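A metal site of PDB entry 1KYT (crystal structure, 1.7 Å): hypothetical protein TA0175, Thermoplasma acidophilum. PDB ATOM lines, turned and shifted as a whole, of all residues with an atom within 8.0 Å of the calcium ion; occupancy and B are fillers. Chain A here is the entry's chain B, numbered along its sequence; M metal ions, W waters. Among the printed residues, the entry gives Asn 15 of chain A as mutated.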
ATOM      1  N   ILE A  10      27.332   4.275 -34.637  1.00  0.00           N
ATOM      2  CA  ILE A  10      26.936   4.374 -33.241  1.00  0.00           C
ATOM      3  C   ILE A  10      25.573   4.948 -32.929  1.00  0.00           C
ATOM      4  O   ILE A  10      25.285   6.073 -33.317  1.00  0.00           O
ATOM      5  CB  ILE A  10      27.972   5.215 -32.462  1.00  0.00           C
ATOM      6  CG1 ILE A  10      29.386   4.713 -32.772  1.00  0.00           C
ATOM      7  CG2 ILE A  10      27.672   5.164 -30.991  1.00  0.00           C
ATOM      8  CD1 ILE A  10      30.487   5.531 -32.124  1.00  0.00           C
ATOM      9  N   ASP A  11      24.755   4.208 -32.200  1.00  0.00           N
ATOM     10  CA  ASP A  11      23.438   4.697 -31.817  1.00  0.00           C
ATOM     11  C   ASP A  11      23.646   5.644 -30.642  1.00  0.00           C
ATOM     12  O   ASP A  11      24.257   5.267 -29.632  1.00  0.00           O
ATOM     13  CB  ASP A  11      22.522   3.559 -31.389  1.00  0.00           C
ATOM     14  CG  ASP A  11      21.291   4.073 -30.679  1.00  0.00           C
ATOM     15  OD1 ASP A  11      20.357   4.604 -31.331  1.00  0.00           O
ATOM     16  OD2 ASP A  11      21.271   3.968 -29.447  1.00  0.00           O
ATOM     17  N   VAL A  12      23.107   6.843 -30.755  1.00  0.00           N
ATOM     18  CA  VAL A  12      23.277   7.864 -29.721  1.00  0.00           C
ATOM     19  C   VAL A  12      22.776   7.559 -28.303  1.00  0.00           C
ATOM     20  O   VAL A  12      23.569   7.505 -27.360  1.00  0.00           O
ATOM     21  CB  VAL A  12      22.647   9.211 -30.175  1.00  0.00           C
ATOM     22  CG1 VAL A  12      22.909  10.286 -29.115  1.00  0.00           C
ATOM     23  CG2 VAL A  12      23.254   9.637 -31.516  1.00  0.00           C
ATOM     24  N   ASP A  13      21.469   7.367 -28.188  1.00  0.00           N
ATOM     25  CA  ASP A  13      20.803   7.125 -26.902  1.00  0.00           C
ATOM     26  C   ASP A  13      21.201   5.825 -26.218  1.00  0.00           C
ATOM     27  O   ASP A  13      21.106   4.747 -26.794  1.00  0.00           O
ATOM     28  CB  ASP A  13      19.287   7.132 -27.124  1.00  0.00           C
ATOM     29  CG  ASP A  13      18.519   7.282 -25.817  1.00  0.00           C
ATOM     30  OD1 ASP A  13      18.543   8.380 -25.237  1.00  0.00           O
ATOM     31  OD2 ASP A  13      17.895   6.288 -25.390  1.00  0.00           O
ATOM     32  N   GLY A  14      21.658   5.933 -24.975  1.00  0.00           N
ATOM     33  CA  GLY A  14      22.058   4.737 -24.258  1.00  0.00           C
ATOM     34  C   GLY A  14      23.508   4.372 -24.503  1.00  0.00           C
ATOM     35  O   GLY A  14      24.068   3.552 -23.786  1.00  0.00           O
ATOM     36  N   ASN A  15      24.117   4.971 -25.518  1.00  0.00           N
ATOM     37  CA  ASN A  15      25.513   4.694 -25.811  1.00  0.00           C
ATOM     38  C   ASN A  15      26.385   5.947 -25.724  1.00  0.00           C
ATOM     39  O   ASN A  15      27.535   5.882 -25.301  1.00  0.00           O
ATOM     40  CB  ASN A  15      25.625   4.074 -27.204  1.00  0.00           C
ATOM     41  CG  ASN A  15      24.747   2.845 -27.336  1.00  0.00           C
ATOM     42  OD1 ASN A  15      25.060   1.803 -26.774  1.00  0.00           O
ATOM     43  ND2 ASN A  15      23.618   2.968 -28.051  1.00  0.00           N
ATOM     44  N   LEU A  16      25.850   7.087 -26.121  1.00  0.00           N
ATOM     45  CA  LEU A  16      26.637   8.303 -26.048  1.00  0.00           C
ATOM     46  C   LEU A  16      26.180   9.201 -24.904  1.00  0.00           C
ATOM     47  O   LEU A  16      26.811  10.214 -24.608  1.00  0.00           O
ATOM     48  CB  LEU A  16      26.569   9.066 -27.377  1.00  0.00           C
ATOM     49  CG  LEU A  16      27.269   8.334 -28.522  1.00  0.00           C
ATOM     50  CD1 LEU A  16      27.293   9.196 -29.767  1.00  0.00           C
ATOM     51  CD2 LEU A  16      28.691   7.970 -28.088  1.00  0.00           C
ATOM     52  N   THR A  17      25.079   8.808 -24.276  1.00  0.00           N
ATOM     53  CA  THR A  17      24.502   9.576 -23.182  1.00  0.00           C
ATOM     54  C   THR A  17      24.883   9.018 -21.813  1.00  0.00           C
ATOM     55  O   THR A  17      25.196   7.846 -21.682  1.00  0.00           O
ATOM     56  CB  THR A  17      22.962   9.609 -23.285  1.00  0.00           C
ATOM     57  OG1 THR A  17      22.454   8.272 -23.241  1.00  0.00           O
ATOM     58  CG2 THR A  17      22.532  10.244 -24.596  1.00  0.00           C
ATOM     59  N   ARG A  21      20.854  11.201 -19.479  1.00  0.00           N
ATOM     60  CA  ARG A  21      20.488  11.259 -20.890  1.00  0.00           C
ATOM     61  C   ARG A  21      21.233  12.411 -21.562  1.00  0.00           C
ATOM     62  O   ARG A  21      20.866  12.861 -22.647  1.00  0.00           O
ATOM     63  CB  ARG A  21      18.981  11.445 -21.049  1.00  0.00           C
ATOM     64  CG  ARG A  21      18.154  10.284 -20.515  1.00  0.00           C
ATOM     65  CD  ARG A  21      18.413   8.990 -21.281  1.00  0.00           C
ATOM     66  NE  ARG A  21      17.609   7.877 -20.769  1.00  0.00           N
ATOM     67  CZ  ARG A  21      17.567   6.659 -21.298  1.00  0.00           C
ATOM     68  NH1 ARG A  21      18.286   6.378 -22.379  1.00  0.00           N
ATOM     69  NH2 ARG A  21      16.793   5.726 -20.759  1.00  0.00           N
ATOM     70  N   LEU A  44      23.601   7.481 -35.348  1.00  0.00           N
ATOM     71  CA  LEU A  44      22.224   7.178 -35.689  1.00  0.00           C
ATOM     72  C   LEU A  44      21.345   7.364 -34.464  1.00  0.00           C
ATOM     73  O   LEU A  44      21.763   7.065 -33.324  1.00  0.00           O
ATOM     74  CB  LEU A  44      22.086   5.735 -36.164  1.00  0.00           C
ATOM     75  CG  LEU A  44      23.030   5.293 -37.274  1.00  0.00           C
ATOM     76  CD1 LEU A  44      24.319   4.816 -36.670  1.00  0.00           C
ATOM     77  CD2 LEU A  44      22.387   4.199 -38.090  1.00  0.00           C
ATOM     78  N   SER A  45      20.134   7.871 -34.687  1.00  0.00           N
ATOM     79  CA  SER A  45      19.187   8.090 -33.601  1.00  0.00           C
ATOM     80  C   SER A  45      17.773   8.367 -34.129  1.00  0.00           C
ATOM     81  O   SER A  45      17.544   8.390 -35.326  1.00  0.00           O
ATOM     82  CB  SER A  45      19.645   9.260 -32.721  1.00  0.00           C
ATOM     83  OG  SER A  45      19.099  10.493 -33.149  1.00  0.00           O
ATOM     84  N   SER A 141      11.337   5.078 -28.240  1.00  0.00           N
ATOM     85  CA  SER A 141      12.786   5.176 -28.122  1.00  0.00           C
ATOM     86  C   SER A 141      13.208   6.626 -28.015  1.00  0.00           C
ATOM     87  O   SER A 141      12.726   7.489 -28.740  1.00  0.00           O
ATOM     88  CB  SER A 141      13.495   4.507 -29.300  1.00  0.00           C
ATOM     89  OG  SER A 141      14.911   4.473 -29.090  1.00  0.00           O
ATOM     90  N   GLY A 142      14.133   6.894 -27.104  1.00  0.00           N
ATOM     91  CA  GLY A 142      14.595   8.259 -26.963  1.00  0.00           C
ATOM     92  C   GLY A 142      13.626   9.215 -26.303  1.00  0.00           C
ATOM     93  O   GLY A 142      13.374   9.124 -25.110  1.00  0.00           O
ATOM     94  N   LYS A 154      17.717   1.097 -38.395  1.00  0.00           N
ATOM     95  CA  LYS A 154      19.148   1.251 -38.386  1.00  0.00           C
ATOM     96  C   LYS A 154      19.894   0.256 -39.256  1.00  0.00           C
ATOM     97  O   LYS A 154      21.037   0.497 -39.627  1.00  0.00           O
ATOM     98  CB  LYS A 154      19.655   1.238 -36.957  1.00  0.00           C
ATOM     99  CG  LYS A 154      19.037   2.320 -36.102  1.00  0.00           C
ATOM    100  CD  LYS A 154      19.920   2.553 -34.869  1.00  0.00           C
ATOM    101  CE  LYS A 154      19.401   3.648 -33.992  1.00  0.00           C
ATOM    102  NZ  LYS A 154      18.370   3.142 -33.064  1.00  0.00           N
ATOM    103  N   ILE A 175      27.697  -0.189 -32.465  1.00  0.00           N
ATOM    104  CA  ILE A 175      27.556  -0.045 -31.019  1.00  0.00           C
ATOM    105  C   ILE A 175      26.112   0.382 -30.702  1.00  0.00           C
ATOM    106  O   ILE A 175      25.635   1.423 -31.188  1.00  0.00           O
ATOM    107  CB  ILE A 175      28.528   1.006 -30.444  1.00  0.00           C
ATOM    108  CG1 ILE A 175      29.971   0.588 -30.757  1.00  0.00           C
ATOM    109  CG2 ILE A 175      28.321   1.132 -28.938  1.00  0.00           C
ATOM    110  CD1 ILE A 175      31.008   1.680 -30.523  1.00  0.00           C
ATOM    111  N   GLY A 176      25.433  -0.432 -29.904  1.00  0.00           N
ATOM    112  CA  GLY A 176      24.050  -0.176 -29.542  1.00  0.00           C
ATOM    113  C   GLY A 176      23.731  -0.803 -28.203  1.00  0.00           C
ATOM    114  O   GLY A 176      24.586  -1.499 -27.625  1.00  0.00           O
ATOM    115  N   ASP A 177      22.528  -0.582 -27.700  1.00  0.00           N
ATOM    116  CA  ASP A 177      22.203  -1.127 -26.388  1.00  0.00           C
ATOM    117  C   ASP A 177      20.750  -1.520 -26.160  1.00  0.00           C
ATOM    118  O   ASP A 177      20.486  -2.330 -25.283  1.00  0.00           O
ATOM    119  CB  ASP A 177      22.548  -0.110 -25.314  1.00  0.00           C
ATOM    120  CG  ASP A 177      21.567   1.032 -25.293  1.00  0.00           C
ATOM    121  OD1 ASP A 177      21.400   1.634 -26.370  1.00  0.00           O
ATOM    122  OD2 ASP A 177      20.962   1.314 -24.253  1.00  0.00           O
ATOM    123  N   SER A 178      19.818  -0.922 -26.896  1.00  0.00           N
ATOM    124  CA  SER A 178      18.409  -1.242 -26.704  1.00  0.00           C
ATOM    125  C   SER A 178      17.806  -2.062 -27.835  1.00  0.00           C
ATOM    126  O   SER A 178      18.466  -2.358 -28.833  1.00  0.00           O
ATOM    127  CB  SER A 178      17.603   0.049 -26.492  1.00  0.00           C
ATOM    128  OG  SER A 178      17.948   1.022 -27.458  1.00  0.00           O
ATOM    129  N   ASN A 179      16.552  -2.428 -27.668  1.00  0.00           N
ATOM    130  CA  ASN A 179      15.882  -3.262 -28.650  1.00  0.00           C
ATOM    131  C   ASN A 179      15.813  -2.696 -30.054  1.00  0.00           C
ATOM    132  O   ASN A 179      15.914  -3.452 -31.000  1.00  0.00           O
ATOM    133  CB  ASN A 179      14.480  -3.640 -28.165  1.00  0.00           C
ATOM    134  CG  ASN A 179      13.847  -4.696 -29.036  1.00  0.00           C
ATOM    135  OD1 ASN A 179      12.977  -4.407 -29.857  1.00  0.00           O
ATOM    136  ND2 ASN A 179      14.285  -5.944 -28.867  1.00  0.00           N
ATOM    137  N   ASN A 180      15.643  -1.389 -30.184  1.00  0.00           N
ATOM    138  CA  ASN A 180      15.559  -0.801 -31.522  1.00  0.00           C
ATOM    139  C   ASN A 180      16.939  -0.691 -32.156  1.00  0.00           C
ATOM    140  O   ASN A 180      17.090  -0.094 -33.220  1.00  0.00           O
ATOM    141  CB  ASN A 180      14.899   0.580 -31.472  1.00  0.00           C
ATOM    142  CG  ASN A 180      15.695   1.572 -30.667  1.00  0.00           C
ATOM    143  OD1 ASN A 180      15.582   2.785 -30.869  1.00  0.00           O
ATOM    144  ND2 ASN A 180      16.511   1.077 -29.755  1.00  0.00           N
ATOM    145  N   ASP A 181      17.929  -1.265 -31.501  1.00  0.00           N
ATOM    146  CA  ASP A 181      19.297  -1.269 -32.000  1.00  0.00           C
ATOM    147  C   ASP A 181      19.607  -2.662 -32.515  1.00  0.00           C
ATOM    148  O   ASP A 181      20.561  -2.853 -33.281  1.00  0.00           O
ATOM    149  CB  ASP A 181      20.305  -0.924 -30.900  1.00  0.00           C
ATOM    150  CG  ASP A 181      20.100   0.464 -30.304  1.00  0.00           C
ATOM    151  OD1 ASP A 181      19.811   1.410 -31.064  1.00  0.00           O
ATOM    152  OD2 ASP A 181      20.246   0.609 -29.072  1.00  0.00           O
ATOM    153  N   MET A 182      18.806  -3.642 -32.095  1.00  0.00           N
ATOM    154  CA  MET A 182      18.985  -5.037 -32.495  1.00  0.00           C
ATOM    155  C   MET A 182      19.127  -5.236 -34.002  1.00  0.00           C
ATOM    156  O   MET A 182      19.860  -6.107 -34.457  1.00  0.00           O
ATOM    157  CB  MET A 182      17.824  -5.906 -31.984  1.00  0.00           C
ATOM    158  CG  MET A 182      17.931  -7.376 -32.379  1.00  0.00           C
ATOM    159  SD  MET A 182      19.620  -8.185 -31.829  1.00  0.00           S
ATOM    160  CE  MET A 182      19.101  -8.768 -30.046  1.00  0.00           C
ATOM    161  N   MET A 184      20.823  -3.643 -36.209  1.00  0.00           N
ATOM    162  CA  MET A 184      22.219  -3.541 -36.645  1.00  0.00           C
ATOM    163  C   MET A 184      22.950  -4.813 -36.269  1.00  0.00           C
ATOM    164  O   MET A 184      23.864  -5.258 -36.989  1.00  0.00           O
ATOM    165  CB  MET A 184      22.951  -2.370 -35.980  1.00  0.00           C
ATOM    166  CG  MET A 184      22.228  -1.047 -36.015  1.00  0.00           C
ATOM    167  SD  MET A 184      23.429   0.429 -35.638  1.00  0.00           S
ATOM    168  CE  MET A 184      23.795   0.093 -33.764  1.00  0.00           C
ATOM    169  N   PRO A 194      27.426  -1.400 -24.365  1.00  0.00           N
ATOM    170  CA  PRO A 194      27.829  -0.957 -23.021  1.00  0.00           C
ATOM    171  C   PRO A 194      27.488  -2.037 -21.977  1.00  0.00           C
ATOM    172  O   PRO A 194      26.766  -2.999 -22.267  1.00  0.00           O
ATOM    173  CB  PRO A 194      27.037   0.342 -22.837  1.00  0.00           C
ATOM    174  CG  PRO A 194      25.798   0.093 -23.632  1.00  0.00           C
ATOM    175  CD  PRO A 194      26.353  -0.531 -24.888  1.00  0.00           C
HETATM  176 CA    CA M   1      19.758   2.837 -27.900  1.00  0.00          CA
HETATM  177  O   HOH W   1      18.064   3.495 -29.664  1.00  0.00           O
HETATM  178  O   HOH W   2      17.969   3.751 -26.260  1.00  0.00           O
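O of Asp 13 sits close to ND2 of Asn 15 (3.3 Å). OG of Ser 178 sits close to ND2 of Asn 180 (2.7 Å). O of Asp 11 sits at hydrogen-bond distance from ND2 of Asn 15 (2.9 Å). The side-chain carboxylate of Asp 13 lies within salt-bridge range of the guanidinium group of Arg 21 (3.0 Å). NZ of Lys 154 lies within salt-bridge range of OD1 of Asp 11 (3.0 Å). The backbone NH of Asp 11 lies within hydrogen-bond range of the backbone carbonyl oxygen of Ile 175 (3.1 Å). OD1 of Asp 181 is in salt-bridge range of NZ of Lys 154 (3.0 Å). The side-chain amide oxygen of Asn 15 sits close to the backbone carbonyl oxygen of Gly 176, at 3.4 Å.
ND2 of Asn 15 touches the calcium ion (3.9 Å). Along chain A the residues within 4 Å of the calcium ion span positions 11 to 181. The nearest printed residue that does not touch the calcium ion is Asn 180 (4.1 Å).
The calcium ion is bound by OD2 of Asp 11 (2.4 Å), water W1 (2.5 Å), OD1 of Asp 177 (2.5 Å), OD2 of Asp 181 (2.6 Å), O of Asp 13 (2.6 Å), water W2 (2.6 Å) and OG of Ser 178 (2.6 Å).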
